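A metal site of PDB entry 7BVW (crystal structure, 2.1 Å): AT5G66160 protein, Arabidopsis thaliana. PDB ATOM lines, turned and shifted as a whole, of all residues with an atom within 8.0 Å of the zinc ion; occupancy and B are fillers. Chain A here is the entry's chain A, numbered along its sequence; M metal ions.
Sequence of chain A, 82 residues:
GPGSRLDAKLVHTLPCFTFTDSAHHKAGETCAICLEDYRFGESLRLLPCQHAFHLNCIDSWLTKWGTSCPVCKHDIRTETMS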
ATOM      1  N   THR A  30     -13.415  28.548 -20.457  1.00  0.00           N
ATOM      2  CA  THR A  30     -13.928  28.311 -21.792  1.00  0.00           C
ATOM      3  C   THR A  30     -12.856  28.612 -22.835  1.00  0.00           C
ATOM      4  O   THR A  30     -12.080  29.561 -22.685  1.00  0.00           O
ATOM      5  CB  THR A  30     -15.173  29.173 -22.051  1.00  0.00           C
ATOM      6  OG1 THR A  30     -16.106  28.988 -20.986  1.00  0.00           O
ATOM      7  CG2 THR A  30     -15.833  28.786 -23.371  1.00  0.00           C
ATOM      8  N   CYS A  31     -12.823  27.805 -23.884  1.00  0.00           N
ATOM      9  CA  CYS A  31     -11.973  28.063 -25.037  1.00  0.00           C
ATOM     10  C   CYS A  31     -12.649  29.079 -25.951  1.00  0.00           C
ATOM     11  O   CYS A  31     -13.768  28.851 -26.414  1.00  0.00           O
ATOM     12  CB  CYS A  31     -11.675  26.773 -25.797  1.00  0.00           C
ATOM     13  SG  CYS A  31     -10.709  27.000 -27.298  1.00  0.00           S
ATOM     14  N   ALA A  32     -11.970  30.204 -26.215  1.00  0.00           N
ATOM     15  CA  ALA A  32     -12.560  31.261 -27.033  1.00  0.00           C
ATOM     16  C   ALA A  32     -12.680  30.873 -28.503  1.00  0.00           C
ATOM     17  O   ALA A  32     -13.445  31.506 -29.237  1.00  0.00           O
ATOM     18  CB  ALA A  32     -11.734  32.542 -26.894  1.00  0.00           C
ATOM     19  N   ILE A  33     -11.935  29.865 -28.950  1.00  0.00           N
ATOM     20  CA  ILE A  33     -11.937  29.505 -30.366  1.00  0.00           C
ATOM     21  C   ILE A  33     -13.160  28.665 -30.730  1.00  0.00           C
ATOM     22  O   ILE A  33     -13.733  28.843 -31.810  1.00  0.00           O
ATOM     23  CB  ILE A  33     -10.618  28.790 -30.715  1.00  0.00           C
ATOM     24  CG1 ILE A  33      -9.429  29.747 -30.544  1.00  0.00           C
ATOM     25  CG2 ILE A  33     -10.656  28.237 -32.137  1.00  0.00           C
ATOM     26  CD1 ILE A  33      -8.101  29.158 -30.951  1.00  0.00           C
ATOM     27  N   CYS A  34     -13.569  27.765 -29.845  1.00  0.00           N
ATOM     28  CA  CYS A  34     -14.719  26.900 -30.107  1.00  0.00           C
ATOM     29  C   CYS A  34     -15.904  27.160 -29.188  1.00  0.00           C
ATOM     30  O   CYS A  34     -16.971  26.593 -29.423  1.00  0.00           O
ATOM     31  CB  CYS A  34     -14.308  25.425 -29.993  1.00  0.00           C
ATOM     32  SG  CYS A  34     -13.894  24.884 -28.321  1.00  0.00           S
ATOM     33  N   LEU A  35     -15.735  28.005 -28.161  1.00  0.00           N
ATOM     34  CA  LEU A  35     -16.768  28.425 -27.216  1.00  0.00           C
ATOM     35  C   LEU A  35     -17.224  27.308 -26.276  1.00  0.00           C
ATOM     36  O   LEU A  35     -18.184  27.500 -25.524  1.00  0.00           O
ATOM     37  CB  LEU A  35     -17.988  29.029 -27.917  1.00  0.00           C
ATOM     38  CG  LEU A  35     -17.748  30.238 -28.823  1.00  0.00           C
ATOM     39  CD1 LEU A  35     -19.076  30.905 -29.165  1.00  0.00           C
ATOM     40  CD2 LEU A  35     -16.777  31.221 -28.188  1.00  0.00           C
ATOM     41  N   GLU A  36     -16.557  26.153 -26.294  1.00  0.00           N
ATOM     42  CA  GLU A  36     -16.903  25.063 -25.400  1.00  0.00           C
ATOM     43  C   GLU A  36     -16.168  25.211 -24.072  1.00  0.00           C
ATOM     44  O   GLU A  36     -14.987  25.581 -24.048  1.00  0.00           O
ATOM     45  CB  GLU A  36     -16.571  23.708 -26.041  1.00  0.00           C
ATOM     46  CG  GLU A  36     -17.175  23.500 -27.416  1.00  0.00           C
ATOM     47  CD  GLU A  36     -18.664  23.240 -27.365  1.00  0.00           C
ATOM     48  OE1 GLU A  36     -19.197  22.977 -26.265  1.00  0.00           O
ATOM     49  OE2 GLU A  36     -19.313  23.286 -28.431  1.00  0.00           O
ATOM     50  N   ASP A  37     -16.860  24.920 -22.980  1.00  0.00           N
ATOM     51  CA  ASP A  37     -16.212  24.923 -21.670  1.00  0.00           C
ATOM     52  C   ASP A  37     -15.217  23.775 -21.577  1.00  0.00           C
ATOM     53  O   ASP A  37     -15.484  22.664 -22.030  1.00  0.00           O
ATOM     54  CB  ASP A  37     -17.254  24.803 -20.555  1.00  0.00           C
ATOM     55  CG  ASP A  37     -18.228  25.966 -20.537  1.00  0.00           C
ATOM     56  OD1 ASP A  37     -17.851  27.060 -21.018  1.00  0.00           O
ATOM     57  OD2 ASP A  37     -19.367  25.797 -20.050  1.00  0.00           O
ATOM     58  N   TYR A  38     -14.059  24.062 -20.973  1.00  0.00           N
ATOM     59  CA  TYR A  38     -13.049  23.021 -20.795  1.00  0.00           C
ATOM     60  C   TYR A  38     -13.610  21.888 -19.947  1.00  0.00           C
ATOM     61  O   TYR A  38     -14.352  22.111 -18.983  1.00  0.00           O
ATOM     62  CB  TYR A  38     -11.798  23.588 -20.136  1.00  0.00           C
ATOM     63  CG  TYR A  38     -11.071  24.667 -20.936  1.00  0.00           C
ATOM     64  CD1 TYR A  38     -10.592  24.413 -22.213  1.00  0.00           C
ATOM     65  CD2 TYR A  38     -10.854  25.919 -20.385  1.00  0.00           C
ATOM     66  CE1 TYR A  38      -9.920  25.396 -22.932  1.00  0.00           C
ATOM     67  CE2 TYR A  38     -10.190  26.911 -21.096  1.00  0.00           C
ATOM     68  CZ  TYR A  38      -9.722  26.644 -22.370  1.00  0.00           C
ATOM     69  OH  TYR A  38      -9.053  27.626 -23.067  1.00  0.00           O
ATOM     70  N   GLU A  42      -8.830  17.460 -20.657  1.00  0.00           N
ATOM     71  CA  GLU A  42      -8.544  17.973 -21.991  1.00  0.00           C
ATOM     72  C   GLU A  42      -7.139  18.553 -22.067  1.00  0.00           C
ATOM     73  O   GLU A  42      -6.538  18.928 -21.059  1.00  0.00           O
ATOM     74  CB  GLU A  42      -9.568  19.024 -22.391  1.00  0.00           C
ATOM     75  CG  GLU A  42     -10.944  18.475 -22.685  1.00  0.00           C
ATOM     76  CD  GLU A  42     -11.919  19.558 -23.097  1.00  0.00           C
ATOM     77  OE1 GLU A  42     -11.660  20.740 -22.769  1.00  0.00           O
ATOM     78  OE2 GLU A  42     -12.929  19.235 -23.745  1.00  0.00           O
ATOM     79  N   SER A  43      -6.614  18.619 -23.287  1.00  0.00           N
ATOM     80  CA  SER A  43      -5.291  19.149 -23.553  1.00  0.00           C
ATOM     81  C   SER A  43      -5.392  20.600 -23.978  1.00  0.00           C
ATOM     82  O   SER A  43      -6.161  20.935 -24.893  1.00  0.00           O
ATOM     83  CB  SER A  43      -4.586  18.332 -24.636  1.00  0.00           C
ATOM     84  OG  SER A  43      -4.258  17.029 -24.164  1.00  0.00           O
ATOM     85  N   LEU A  44      -4.624  21.461 -23.324  1.00  0.00           N
ATOM     86  CA  LEU A  44      -4.619  22.886 -23.603  1.00  0.00           C
ATOM     87  C   LEU A  44      -3.223  23.342 -23.990  1.00  0.00           C
ATOM     88  O   LEU A  44      -2.231  22.676 -23.715  1.00  0.00           O
ATOM     89  CB  LEU A  44      -5.111  23.703 -22.399  1.00  0.00           C
ATOM     90  CG  LEU A  44      -6.614  23.942 -22.229  1.00  0.00           C
ATOM     91  CD1 LEU A  44      -7.369  22.654 -21.956  1.00  0.00           C
ATOM     92  CD2 LEU A  44      -6.835  24.939 -21.112  1.00  0.00           C
ATOM     93  N   ALA A  52      -4.944  30.891 -22.889  1.00  0.00           N
ATOM     94  CA  ALA A  52      -4.891  29.454 -23.135  1.00  0.00           C
ATOM     95  C   ALA A  52      -6.090  29.014 -23.955  1.00  0.00           C
ATOM     96  O   ALA A  52      -7.151  29.641 -23.946  1.00  0.00           O
ATOM     97  CB  ALA A  52      -4.846  28.672 -21.816  1.00  0.00           C
ATOM     98  N   PHE A  53      -5.893  27.916 -24.687  1.00  0.00           N
ATOM     99  CA  PHE A  53      -6.924  27.383 -25.560  1.00  0.00           C
ATOM    100  C   PHE A  53      -6.838  25.871 -25.571  1.00  0.00           C
ATOM    101  O   PHE A  53      -5.865  25.281 -25.093  1.00  0.00           O
ATOM    102  CB  PHE A  53      -6.790  27.901 -27.000  1.00  0.00           C
ATOM    103  CG  PHE A  53      -6.659  29.396 -27.107  1.00  0.00           C
ATOM    104  CD1 PHE A  53      -5.416  30.007 -27.005  1.00  0.00           C
ATOM    105  CD2 PHE A  53      -7.775  30.176 -27.346  1.00  0.00           C
ATOM    106  CE1 PHE A  53      -5.308  31.382 -27.109  1.00  0.00           C
ATOM    107  CE2 PHE A  53      -7.653  31.555 -27.453  1.00  0.00           C
ATOM    108  CZ  PHE A  53      -6.419  32.153 -27.334  1.00  0.00           C
ATOM    109  N   HIS A  54      -7.876  25.231 -26.120  1.00  0.00           N
ATOM    110  CA  HIS A  54      -7.757  23.853 -26.541  1.00  0.00           C
ATOM    111  C   HIS A  54      -6.541  23.715 -27.458  1.00  0.00           C
ATOM    112  O   HIS A  54      -6.340  24.543 -28.353  1.00  0.00           O
ATOM    113  CB  HIS A  54      -9.024  23.407 -27.274  1.00  0.00           C
ATOM    114  CG  HIS A  54     -10.160  23.030 -26.367  1.00  0.00           C
ATOM    115  ND1 HIS A  54     -11.467  23.382 -26.627  1.00  0.00           N
ATOM    116  CD2 HIS A  54     -10.180  22.326 -25.219  1.00  0.00           C
ATOM    117  CE1 HIS A  54     -12.249  22.916 -25.668  1.00  0.00           C
ATOM    118  NE2 HIS A  54     -11.487  22.271 -24.795  1.00  0.00           N
ATOM    119  N   LEU A  55      -5.735  22.684 -27.214  1.00  0.00           N
ATOM    120  CA  LEU A  55      -4.530  22.480 -28.017  1.00  0.00           C
ATOM    121  C   LEU A  55      -4.868  22.369 -29.496  1.00  0.00           C
ATOM    122  O   LEU A  55      -4.238  23.013 -30.344  1.00  0.00           O
ATOM    123  CB  LEU A  55      -3.774  21.240 -27.530  1.00  0.00           C
ATOM    124  CG  LEU A  55      -2.474  20.873 -28.251  1.00  0.00           C
ATOM    125  CD1 LEU A  55      -1.474  20.347 -27.246  1.00  0.00           C
ATOM    126  CD2 LEU A  55      -2.712  19.826 -29.342  1.00  0.00           C
ATOM    127  N   ASN A  56      -5.883  21.558 -29.833  1.00  0.00           N
ATOM    128  CA  ASN A  56      -6.256  21.386 -31.236  1.00  0.00           C
ATOM    129  C   ASN A  56      -6.808  22.677 -31.827  1.00  0.00           C
ATOM    130  O   ASN A  56      -6.632  22.946 -33.018  1.00  0.00           O
ATOM    131  CB  ASN A  56      -7.283  20.262 -31.369  1.00  0.00           C
ATOM    132  CG  ASN A  56      -6.649  18.893 -31.335  1.00  0.00           C
ATOM    133  OD1 ASN A  56      -5.477  18.739 -31.663  1.00  0.00           O
ATOM    134  ND2 ASN A  56      -7.437  17.885 -30.966  1.00  0.00           N
ATOM    135  N   CYS A  57      -7.491  23.492 -31.016  1.00  0.00           N
ATOM    136  CA  CYS A  57      -8.098  24.707 -31.533  1.00  0.00           C
ATOM    137  C   CYS A  57      -7.045  25.749 -31.909  1.00  0.00           C
ATOM    138  O   CYS A  57      -7.075  26.307 -33.005  1.00  0.00           O
ATOM    139  CB  CYS A  57      -9.085  25.282 -30.511  1.00  0.00           C
ATOM    140  SG  CYS A  57     -10.592  24.316 -30.346  1.00  0.00           S
ATOM    141  N   ILE A  58      -6.096  26.014 -31.000  1.00  0.00           N
ATOM    142  CA  ILE A  58      -5.103  27.041 -31.261  1.00  0.00           C
ATOM    143  C   ILE A  58      -4.092  26.565 -32.300  1.00  0.00           C
ATOM    144  O   ILE A  58      -3.587  27.374 -33.093  1.00  0.00           O
ATOM    145  CB  ILE A  58      -4.410  27.466 -29.950  1.00  0.00           C
ATOM    146  CG1 ILE A  58      -3.520  28.694 -30.184  1.00  0.00           C
ATOM    147  CG2 ILE A  58      -3.607  26.319 -29.347  1.00  0.00           C
ATOM    148  CD1 ILE A  58      -4.292  29.910 -30.674  1.00  0.00           C
HETATM  149 ZN    ZN M   1     -11.532  24.955 -28.273  1.00  0.00          ZN
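A ring nitrogen (NE2) of His 54 is in hydrogen-bond range of the side-chain carboxylate of Glu 42.
N of Glu 36 sits close to SG of Cys 34.
The backbone NH (N) of Ile 33 sits close to the side-chain sulfur (SG) of Cys 31, 3.5 Å away.
The backbone NH of Cys 31 sits at hydrogen-bond distance from the backbone carbonyl oxygen of Glu 36 (3.1 Å).
Four residues have an atom within 4 Å of the zinc ion: Cys 31, Cys 34, His 54 and Cys 57.
The nearest printed residue that does not touch the zinc ion is Ile 33 (4.6 Å).
The zinc ion is bound by ND1 of His 54, SG of Cys 34, SG of Cys 57 and SG of Cys 31.
The zinc ion has four donor atoms within binding distance.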
